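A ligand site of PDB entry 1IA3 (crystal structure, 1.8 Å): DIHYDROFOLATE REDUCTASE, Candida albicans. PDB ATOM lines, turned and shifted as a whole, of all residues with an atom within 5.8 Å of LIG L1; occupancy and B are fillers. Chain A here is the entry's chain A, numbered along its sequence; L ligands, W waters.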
ATOM      1  N   ILE A   9      -7.243 -13.936  -2.443  1.00  0.00           N
ATOM      2  CA  ILE A   9      -7.210 -13.962  -3.933  1.00  0.00           C
ATOM      3  C   ILE A   9      -5.895 -13.261  -4.334  1.00  0.00           C
ATOM      4  O   ILE A   9      -5.638 -12.155  -3.870  1.00  0.00           O
ATOM      5  CB  ILE A   9      -8.505 -13.313  -4.500  1.00  0.00           C
ATOM      6  CG1 ILE A   9      -8.454 -13.322  -6.058  1.00  0.00           C
ATOM      7  CG2 ILE A   9      -8.740 -11.865  -4.004  1.00  0.00           C
ATOM      8  CD1 ILE A   9      -9.871 -13.091  -6.719  1.00  0.00           C
ATOM      9  N   VAL A  10      -5.113 -13.959  -5.186  1.00  0.00           N
ATOM     10  CA  VAL A  10      -3.801 -13.474  -5.596  1.00  0.00           C
ATOM     11  C   VAL A  10      -3.430 -14.027  -7.002  1.00  0.00           C
ATOM     12  O   VAL A  10      -3.964 -15.042  -7.393  1.00  0.00           O
ATOM     13  CB  VAL A  10      -2.752 -13.969  -4.560  1.00  0.00           C
ATOM     14  CG1 VAL A  10      -2.753 -15.493  -4.419  1.00  0.00           C
ATOM     15  CG2 VAL A  10      -1.369 -13.437  -4.795  1.00  0.00           C
ATOM     16  N   ALA A  11      -2.550 -13.275  -7.615  1.00  0.00           N
ATOM     17  CA  ALA A  11      -2.010 -13.646  -8.973  1.00  0.00           C
ATOM     18  C   ALA A  11      -0.508 -13.833  -8.749  1.00  0.00           C
ATOM     19  O   ALA A  11       0.133 -12.919  -8.245  1.00  0.00           O
ATOM     20  CB  ALA A  11      -2.333 -12.511  -9.911  1.00  0.00           C
ATOM     21  N   ILE A  19       5.039 -12.127  -6.769  1.00  0.00           N
ATOM     22  CA  ILE A  19       3.809 -11.334  -6.818  1.00  0.00           C
ATOM     23  C   ILE A  19       3.970  -9.862  -7.100  1.00  0.00           C
ATOM     24  O   ILE A  19       2.997  -9.134  -7.316  1.00  0.00           O
ATOM     25  CB  ILE A  19       2.940 -11.546  -5.495  1.00  0.00           C
ATOM     26  CG1 ILE A  19       3.827 -11.295  -4.233  1.00  0.00           C
ATOM     27  CG2 ILE A  19       2.364 -13.005  -5.440  1.00  0.00           C
ATOM     28  CD1 ILE A  19       2.906 -11.137  -2.931  1.00  0.00           C
ATOM     29  N   GLY A  20       5.219  -9.379  -7.034  1.00  0.00           N
ATOM     30  CA  GLY A  20       5.419  -7.932  -7.195  1.00  0.00           C
ATOM     31  C   GLY A  20       6.889  -7.545  -7.273  1.00  0.00           C
ATOM     32  O   GLY A  20       7.834  -8.314  -7.034  1.00  0.00           O
ATOM     33  N   TYR A  21       6.986  -6.284  -7.597  1.00  0.00           N
ATOM     34  CA  TYR A  21       8.243  -5.563  -7.743  1.00  0.00           C
ATOM     35  C   TYR A  21       8.074  -4.107  -7.375  1.00  0.00           C
ATOM     36  O   TYR A  21       7.455  -3.336  -8.106  1.00  0.00           O
ATOM     37  CB  TYR A  21       8.744  -5.704  -9.201  1.00  0.00           C
ATOM     38  CG  TYR A  21      10.125  -5.096  -9.368  1.00  0.00           C
ATOM     39  CD1 TYR A  21      10.323  -3.879 -10.011  1.00  0.00           C
ATOM     40  CD2 TYR A  21      11.210  -5.737  -8.796  1.00  0.00           C
ATOM     41  CE1 TYR A  21      11.616  -3.359 -10.125  1.00  0.00           C
ATOM     42  CE2 TYR A  21      12.489  -5.210  -8.867  1.00  0.00           C
ATOM     43  CZ  TYR A  21      12.679  -4.012  -9.536  1.00  0.00           C
ATOM     44  OH  TYR A  21      13.995  -3.569  -9.609  1.00  0.00           O
ATOM     45  N   GLY A  23       6.346  -2.590  -5.076  1.00  0.00           N
ATOM     46  CA  GLY A  23       4.973  -2.211  -4.832  1.00  0.00           C
ATOM     47  C   GLY A  23       3.989  -2.430  -5.948  1.00  0.00           C
ATOM     48  O   GLY A  23       2.791  -2.117  -5.703  1.00  0.00           O
ATOM     49  N   LYS A  24       4.443  -3.013  -7.054  1.00  0.00           N
ATOM     50  CA  LYS A  24       3.563  -3.229  -8.220  1.00  0.00           C
ATOM     51  C   LYS A  24       3.609  -4.570  -8.847  1.00  0.00           C
ATOM     52  O   LYS A  24       4.612  -5.303  -8.781  1.00  0.00           O
ATOM     53  CB  LYS A  24       3.729  -2.072  -9.218  1.00  0.00           C
ATOM     54  CG  LYS A  24       5.154  -1.683  -9.651  1.00  0.00           C
ATOM     55  CD  LYS A  24       5.731  -2.656 -10.661  1.00  0.00           C
ATOM     56  CE  LYS A  24       7.134  -2.441 -11.160  1.00  0.00           C
ATOM     57  NZ  LYS A  24       7.357  -3.392 -12.338  1.00  0.00           N
ATOM     58  N   MET A  25       2.508  -4.924  -9.534  1.00  0.00           N
ATOM     59  CA  MET A  25       2.512  -6.229 -10.264  1.00  0.00           C
ATOM     60  C   MET A  25       3.408  -6.017 -11.499  1.00  0.00           C
ATOM     61  O   MET A  25       3.249  -5.035 -12.240  1.00  0.00           O
ATOM     62  CB  MET A  25       1.132  -6.725 -10.636  1.00  0.00           C
ATOM     63  CG  MET A  25       0.222  -6.806  -9.424  1.00  0.00           C
ATOM     64  SD  MET A  25      -1.458  -7.293  -9.972  1.00  0.00           S
ATOM     65  CE  MET A  25      -1.269  -9.008 -10.159  1.00  0.00           C
ATOM     66  N   GLU A  32      -7.312 -10.719 -16.424  1.00  0.00           N
ATOM     67  CA  GLU A  32      -7.168 -11.142 -14.982  1.00  0.00           C
ATOM     68  C   GLU A  32      -7.717 -10.065 -14.069  1.00  0.00           C
ATOM     69  O   GLU A  32      -8.346 -10.435 -13.079  1.00  0.00           O
ATOM     70  CB  GLU A  32      -5.670 -11.327 -14.686  1.00  0.00           C
ATOM     71  CG  GLU A  32      -5.298 -12.433 -13.648  1.00  0.00           C
ATOM     72  CD  GLU A  32      -5.585 -11.993 -12.235  1.00  0.00           C
ATOM     73  OE1 GLU A  32      -5.474 -10.827 -11.933  1.00  0.00           O
ATOM     74  OE2 GLU A  32      -6.023 -12.878 -11.468  1.00  0.00           O
ATOM     75  N   ILE A  33      -7.508  -8.787 -14.344  1.00  0.00           N
ATOM     76  CA  ILE A  33      -8.060  -7.696 -13.537  1.00  0.00           C
ATOM     77  C   ILE A  33      -9.600  -7.777 -13.547  1.00  0.00           C
ATOM     78  O   ILE A  33     -10.246  -7.538 -12.537  1.00  0.00           O
ATOM     79  CB  ILE A  33      -7.593  -6.287 -14.100  1.00  0.00           C
ATOM     80  CG1 ILE A  33      -6.089  -6.195 -14.106  1.00  0.00           C
ATOM     81  CG2 ILE A  33      -8.290  -5.102 -13.337  1.00  0.00           C
ATOM     82  CD1 ILE A  33      -5.167  -6.409 -12.998  1.00  0.00           C
ATOM     83  N   TYR A  35     -11.506 -10.446 -13.993  1.00  0.00           N
ATOM     84  CA  TYR A  35     -11.896 -11.618 -13.169  1.00  0.00           C
ATOM     85  C   TYR A  35     -11.861 -11.190 -11.676  1.00  0.00           C
ATOM     86  O   TYR A  35     -12.814 -11.446 -10.971  1.00  0.00           O
ATOM     87  CB  TYR A  35     -10.885 -12.738 -13.391  1.00  0.00           C
ATOM     88  CG  TYR A  35     -10.902 -13.911 -12.457  1.00  0.00           C
ATOM     89  CD1 TYR A  35     -10.016 -14.044 -11.379  1.00  0.00           C
ATOM     90  CD2 TYR A  35     -11.899 -14.871 -12.621  1.00  0.00           C
ATOM     91  CE1 TYR A  35     -10.097 -15.144 -10.510  1.00  0.00           C
ATOM     92  CE2 TYR A  35     -11.951 -16.005 -11.803  1.00  0.00           C
ATOM     93  CZ  TYR A  35     -11.067 -16.105 -10.751  1.00  0.00           C
ATOM     94  OH  TYR A  35     -11.168 -17.290 -10.039  1.00  0.00           O
ATOM     95  N   PHE A  36     -10.784 -10.566 -11.286  1.00  0.00           N
ATOM     96  CA  PHE A  36     -10.618 -10.052  -9.905  1.00  0.00           C
ATOM     97  C   PHE A  36     -11.826  -9.213  -9.542  1.00  0.00           C
ATOM     98  O   PHE A  36     -12.387  -9.400  -8.434  1.00  0.00           O
ATOM     99  CB  PHE A  36      -9.265  -9.347  -9.683  1.00  0.00           C
ATOM    100  CG  PHE A  36      -9.151  -8.598  -8.359  1.00  0.00           C
ATOM    101  CD1 PHE A  36      -9.467  -7.238  -8.318  1.00  0.00           C
ATOM    102  CD2 PHE A  36      -8.875  -9.302  -7.176  1.00  0.00           C
ATOM    103  CE1 PHE A  36      -9.454  -6.513  -7.096  1.00  0.00           C
ATOM    104  CE2 PHE A  36      -8.817  -8.573  -5.963  1.00  0.00           C
ATOM    105  CZ  PHE A  36      -9.110  -7.210  -5.916  1.00  0.00           C
ATOM    106  N   THR A  58      -1.041  -1.142   0.540  1.00  0.00           N
ATOM    107  CA  THR A  58      -1.852  -1.412  -0.670  1.00  0.00           C
ATOM    108  C   THR A  58      -2.883  -0.313  -0.844  1.00  0.00           C
ATOM    109  O   THR A  58      -2.983   0.250  -1.928  1.00  0.00           O
ATOM    110  CB  THR A  58      -2.474  -2.871  -0.690  1.00  0.00           C
ATOM    111  OG1 THR A  58      -1.273  -3.729  -0.789  1.00  0.00           O
ATOM    112  CG2 THR A  58      -3.370  -3.103  -1.943  1.00  0.00           C
ATOM    113  N   ILE A 111      -9.332 -11.491   1.095  1.00  0.00           N
ATOM    114  CA  ILE A 111      -8.030 -10.810   1.424  1.00  0.00           C
ATOM    115  C   ILE A 111      -7.405 -10.545   0.041  1.00  0.00           C
ATOM    116  O   ILE A 111      -7.169 -11.490  -0.717  1.00  0.00           O
ATOM    117  CB  ILE A 111      -7.145 -11.706   2.340  1.00  0.00           C
ATOM    118  CG1 ILE A 111      -7.838 -11.874   3.695  1.00  0.00           C
ATOM    119  CG2 ILE A 111      -5.684 -11.136   2.404  1.00  0.00           C
ATOM    120  CD1 ILE A 111      -7.146 -12.982   4.542  1.00  0.00           C
ATOM    121  N   ILE A 112      -7.141  -9.266  -0.212  1.00  0.00           N
ATOM    122  CA  ILE A 112      -6.596  -8.881  -1.532  1.00  0.00           C
ATOM    123  C   ILE A 112      -5.170  -8.499  -1.611  1.00  0.00           C
ATOM    124  O   ILE A 112      -4.643  -8.372  -2.753  1.00  0.00           O
ATOM    125  CB  ILE A 112      -7.569  -7.858  -2.239  1.00  0.00           C
ATOM    126  CG1 ILE A 112      -7.464  -6.464  -1.566  1.00  0.00           C
ATOM    127  CG2 ILE A 112      -9.029  -8.429  -2.303  1.00  0.00           C
ATOM    128  CD1 ILE A 112      -8.067  -5.292  -2.472  1.00  0.00           C
ATOM    129  N   GLY A 113      -4.436  -8.394  -0.511  1.00  0.00           N
ATOM    130  CA  GLY A 113      -3.054  -8.056  -0.502  1.00  0.00           C
ATOM    131  C   GLY A 113      -2.744  -6.989   0.549  1.00  0.00           C
ATOM    132  O   GLY A 113      -3.640  -6.614   1.246  1.00  0.00           O
ATOM    133  N   GLY A 114      -1.475  -6.542   0.609  1.00  0.00           N
ATOM    134  CA  GLY A 114      -0.418  -7.031  -0.270  1.00  0.00           C
ATOM    135  C   GLY A 114       0.406  -8.146   0.316  1.00  0.00           C
ATOM    136  O   GLY A 114      -0.112  -9.028   1.024  1.00  0.00           O
ATOM    137  N   ALA A 115       1.726  -8.087   0.028  1.00  0.00           N
ATOM    138  CA  ALA A 115       2.665  -9.171   0.371  1.00  0.00           C
ATOM    139  C   ALA A 115       2.703  -9.555   1.824  1.00  0.00           C
ATOM    140  O   ALA A 115       2.601 -10.744   2.197  1.00  0.00           O
ATOM    141  CB  ALA A 115       4.037  -8.899  -0.195  1.00  0.00           C
ATOM    142  N   TYR A 118      -0.727 -11.139   2.897  1.00  0.00           N
ATOM    143  CA  TYR A 118      -0.821 -12.508   2.434  1.00  0.00           C
ATOM    144  C   TYR A 118      -0.048 -13.504   3.296  1.00  0.00           C
ATOM    145  O   TYR A 118      -0.580 -14.525   3.713  1.00  0.00           O
ATOM    146  CB  TYR A 118      -0.296 -12.731   0.967  1.00  0.00           C
ATOM    147  CG  TYR A 118      -1.059 -12.071  -0.152  1.00  0.00           C
ATOM    148  CD1 TYR A 118      -2.464 -12.071  -0.232  1.00  0.00           C
ATOM    149  CD2 TYR A 118      -0.350 -11.522  -1.191  1.00  0.00           C
ATOM    150  CE1 TYR A 118      -3.120 -11.521  -1.339  1.00  0.00           C
ATOM    151  CE2 TYR A 118      -0.952 -10.911  -2.277  1.00  0.00           C
ATOM    152  CZ  TYR A 118      -2.357 -10.947  -2.351  1.00  0.00           C
ATOM    153  OH  TYR A 118      -2.917 -10.394  -3.455  1.00  0.00           O
ATOM    154  N   LEU A 131      -7.752 -18.473  -3.934  1.00  0.00           N
ATOM    155  CA  LEU A 131      -8.047 -18.277  -5.377  1.00  0.00           C
ATOM    156  C   LEU A 131      -6.708 -17.716  -5.942  1.00  0.00           C
ATOM    157  O   LEU A 131      -6.419 -16.572  -5.698  1.00  0.00           O
ATOM    158  CB  LEU A 131      -9.242 -17.341  -5.542  1.00  0.00           C
ATOM    159  CG  LEU A 131     -10.572 -17.865  -5.028  1.00  0.00           C
ATOM    160  CD1 LEU A 131     -11.556 -16.707  -4.840  1.00  0.00           C
ATOM    161  CD2 LEU A 131     -11.136 -18.854  -6.039  1.00  0.00           C
ATOM    162  N   THR A 133      -4.262 -17.182  -9.159  1.00  0.00           N
ATOM    163  CA  THR A 133      -4.151 -17.184 -10.667  1.00  0.00           C
ATOM    164  C   THR A 133      -2.688 -17.612 -10.907  1.00  0.00           C
ATOM    165  O   THR A 133      -1.787 -16.869 -10.456  1.00  0.00           O
ATOM    166  CB  THR A 133      -4.419 -15.797 -11.261  1.00  0.00           C
ATOM    167  OG1 THR A 133      -5.751 -15.372 -10.909  1.00  0.00           O
ATOM    168  CG2 THR A 133      -4.264 -15.834 -12.812  1.00  0.00           C
ATOM    169  N   THR A 147       9.032  -9.540  -4.279  1.00  0.00           N
ATOM    170  CA  THR A 147       8.136 -10.140  -3.280  1.00  0.00           C
ATOM    171  C   THR A 147       7.594 -11.457  -3.797  1.00  0.00           C
ATOM    172  O   THR A 147       7.392 -11.645  -4.986  1.00  0.00           O
ATOM    173  CB  THR A 147       6.997  -9.232  -2.746  1.00  0.00           C
ATOM    174  OG1 THR A 147       6.246  -8.795  -3.917  1.00  0.00           O
ATOM    175  CG2 THR A 147       7.448  -8.009  -1.916  1.00  0.00           C
HETATM  176  C1  LIG L   1      -5.560  -8.965  -8.938  1.00  0.00           C
HETATM  177  C2  LIG L   1      -5.426  -8.603  -7.574  1.00  0.00           C
HETATM  178  C3  LIG L   1      -5.482  -9.765  -6.625  1.00  0.00           C
HETATM  179  N1  LIG L   1      -5.620 -10.967  -7.009  1.00  0.00           N
HETATM  180  C4  LIG L   1      -5.856 -11.304  -8.298  1.00  0.00           C
HETATM  181  N2  LIG L   1      -5.680 -10.343  -9.301  1.00  0.00           N
HETATM  182  N3  LIG L   1      -5.461  -9.645  -5.287  1.00  0.00           N
HETATM  183  C5  LIG L   1      -5.549  -7.967  -9.930  1.00  0.00           C
HETATM  184  C6  LIG L   1      -5.363  -6.656  -9.607  1.00  0.00           C
HETATM  185  C7  LIG L   1      -5.244  -6.248  -8.280  1.00  0.00           C
HETATM  186  C8  LIG L   1      -5.255  -7.256  -7.266  1.00  0.00           C
HETATM  187  N4  LIG L   1      -5.962 -12.567  -8.665  1.00  0.00           N
HETATM  188  S1  LIG L   1      -5.123  -6.601  -5.627  1.00  0.00           S
HETATM  189  C9  LIG L   1      -3.329  -6.704  -5.348  1.00  0.00           C
HETATM  190  C10 LIG L   1      -2.393  -7.469  -6.028  1.00  0.00           C
HETATM  191  C11 LIG L   1      -1.030  -7.587  -5.762  1.00  0.00           C
HETATM  192  C12 LIG L   1      -0.436  -6.776  -4.691  1.00  0.00           C
HETATM  193  C13 LIG L   1      -1.367  -6.057  -4.013  1.00  0.00           C
HETATM  194  C14 LIG L   1      -2.745  -5.961  -4.293  1.00  0.00           C
HETATM  195  C15 LIG L   1       1.064  -6.767  -4.515  1.00  0.00           C
HETATM  196  C16 LIG L   1       1.668  -6.148  -3.243  1.00  0.00           C
HETATM  197  C17 LIG L   1       1.565  -8.194  -4.648  1.00  0.00           C
HETATM  198  C18 LIG L   1       1.771  -5.857  -5.634  1.00  0.00           C
HETATM  199  P1  LG2 L   2       0.657  -4.542   2.468  1.00  0.00           P
HETATM  200  O1  LG2 L   2       0.705  -5.912   2.808  1.00  0.00           O
HETATM  201  O2  LG2 L   2      -0.431  -4.043   1.635  1.00  0.00           O
HETATM  202  O3  LG2 L   2       0.630  -3.586   3.787  1.00  0.00           O
HETATM  203  C1  LG2 L   2       1.499  -3.952   4.893  1.00  0.00           C
HETATM  204  C2  LG2 L   2       0.943  -3.097   6.056  1.00  0.00           C
HETATM  205  O4  LG2 L   2      -0.318  -3.644   6.469  1.00  0.00           O
HETATM  206  C3  LG2 L   2       1.857  -3.185   7.317  1.00  0.00           C
HETATM  207  O5  LG2 L   2       2.868  -2.161   7.135  1.00  0.00           O
HETATM  208  C4  LG2 L   2       0.772  -2.863   8.409  1.00  0.00           C
HETATM  209  O6  LG2 L   2       0.286  -1.499   8.376  1.00  0.00           O
HETATM  210  C5  LG2 L   2      -0.431  -3.642   7.844  1.00  0.00           C
HETATM  211  N1  LG2 L   2      -0.416  -4.972   8.358  1.00  0.00           N
HETATM  212  C6  LG2 L   2       0.379  -5.968   7.830  1.00  0.00           C
HETATM  213  N2  LG2 L   2       0.203  -7.125   8.468  1.00  0.00           N
HETATM  214  C7  LG2 L   2      -0.756  -6.807   9.404  1.00  0.00           C
HETATM  215  C8  LG2 L   2      -1.302  -7.648  10.388  1.00  0.00           C
HETATM  216  N3  LG2 L   2      -0.952  -8.953  10.455  1.00  0.00           N
HETATM  217  N4  LG2 L   2      -2.220  -7.063  11.204  1.00  0.00           N
HETATM  218  C9  LG2 L   2      -2.504  -5.736  11.038  1.00  0.00           C
HETATM  219  N5  LG2 L   2      -2.015  -4.872  10.195  1.00  0.00           N
HETATM  220  C10 LG2 L   2      -1.134  -5.505   9.364  1.00  0.00           C
HETATM  221  O7  LG2 L   2       2.004  -4.043   1.801  1.00  0.00           O
HETATM  222  P2  LG2 L   2       3.248  -4.822   1.151  1.00  0.00           P
HETATM  223  O8  LG2 L   2       2.789  -5.319  -0.201  1.00  0.00           O
HETATM  224  O9  LG2 L   2       3.799  -5.877   2.002  1.00  0.00           O
HETATM  225  O10 LG2 L   2       4.317  -3.668   0.944  1.00  0.00           O
HETATM  226  C11 LG2 L   2       4.419  -2.926  -0.273  1.00  0.00           C
HETATM  227  C12 LG2 L   2       5.754  -2.150  -0.206  1.00  0.00           C
HETATM  228  O11 LG2 L   2       6.865  -3.065  -0.443  1.00  0.00           O
HETATM  229  C13 LG2 L   2       5.856  -0.941  -1.068  1.00  0.00           C
HETATM  230  P3  LG2 L   2       1.072  -0.542   9.457  1.00  0.00           P
HETATM  231  O12 LG2 L   2       0.239   0.747   9.325  1.00  0.00           O
HETATM  232  O13 LG2 L   2       1.087  -1.265  10.701  1.00  0.00           O
HETATM  233  O14 LG2 L   2       2.441  -0.377   8.902  1.00  0.00           O
HETATM  234  O   HOH W   1      -2.006 -10.597  -6.597  1.00  0.00           O
HETATM  235  O   HOH W   2       0.307 -10.178  -7.648  1.00  0.00           O
HETATM  236  O   HOH W   3      -7.163 -15.633  -8.539  1.00  0.00           O
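The side-chain carboxylate (OE1) of Glu 32 sits at hydrogen-bond distance from a nitrogen (N2) of LIG L1 (2.7 Å). O of Ile 9 lies within hydrogen-bond range of N3 of LIG L1 (2.9 Å). O of Ile 112 is in hydrogen-bond range of N3 of LIG L1, at 3.0 Å. The side-chain hydroxyl (OH) of Tyr 118 sits at hydrogen-bond distance from a nitrogen (N3) of LIG L1 (3.2 Å). O of Val 10 lies close to N4 of LIG L1 (3.4 Å). The backbone NH (N) of Gly 114 lies within hydrogen-bond range of an oxygen (O2) of LG2 L2, 2.9 Å away. The backbone NH (N) of Thr 58 is in hydrogen-bond range of an oxygen (O2) of LG2 L2 (3.2 Å). O2 of LG2 L2 lies within hydrogen-bond range of OG1 of Thr 58 (2.6 Å). An oxygen (O8) of LG2 L2 is in hydrogen-bond range of the backbone NH (N) of Ala 115 (3.0 Å).
The side-chain hydroxyl (OG1) of Thr 133 sits at hydrogen-bond distance from the side-chain carboxylate (OE2) of Glu 32, 2.6 Å away. O of Ile 9 sits at hydrogen-bond distance from OH of Tyr 118 (3.3 Å). O of Ile 111 is in hydrogen-bond range of N of Ile 9 (3.0 Å). The side-chain hydroxyl (OH) of Tyr 118 is in hydrogen-bond range of the backbone carbonyl oxygen (O) of Ile 112, 2.7 Å away. N of Ile 19 lies within hydrogen-bond range of O of Thr 147 (3.0 Å). The backbone carbonyl oxygen of Val 10 sits at hydrogen-bond distance from the backbone NH of Thr 133, 2.8 Å away. The backbone carbonyl oxygen of Leu 131 lies within hydrogen-bond range of the backbone NH of Val 10 (3.0 Å). OG1 of Thr 58 sits at hydrogen-bond distance from N of Gly 114, 3.1 Å away.
Merely in contact with LIG L1: Ala 11, Ile 19, Gly 23, Lys 24, Met 25, Ile 33, Phe 36, Thr 58, Gly 114, Ala 115 and Thr 133. Hydrophobic or aromatic side chains that line LIG L1: Ile 9, Ala 11, Ile 19, Met 25, Ile 33 and Phe 36.
Water W1 lies within hydrogen-bond range of N of Ala 11 and OH of Tyr 118. Water W3 lies within hydrogen-bond range of the side-chain hydroxyl of Thr 133 (2.8 Å), the backbone carbonyl oxygen of Leu 131 (3.1 Å), a nitrogen (N4) of LIG L1 (3.3 Å) and the backbone carbonyl oxygen of Val 10 (3.4 Å). Water W2 lies within hydrogen-bond range of the backbone carbonyl oxygen of Ala 11 (2.8 Å) and the backbone carbonyl oxygen of Ile 19 (2.9 Å).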
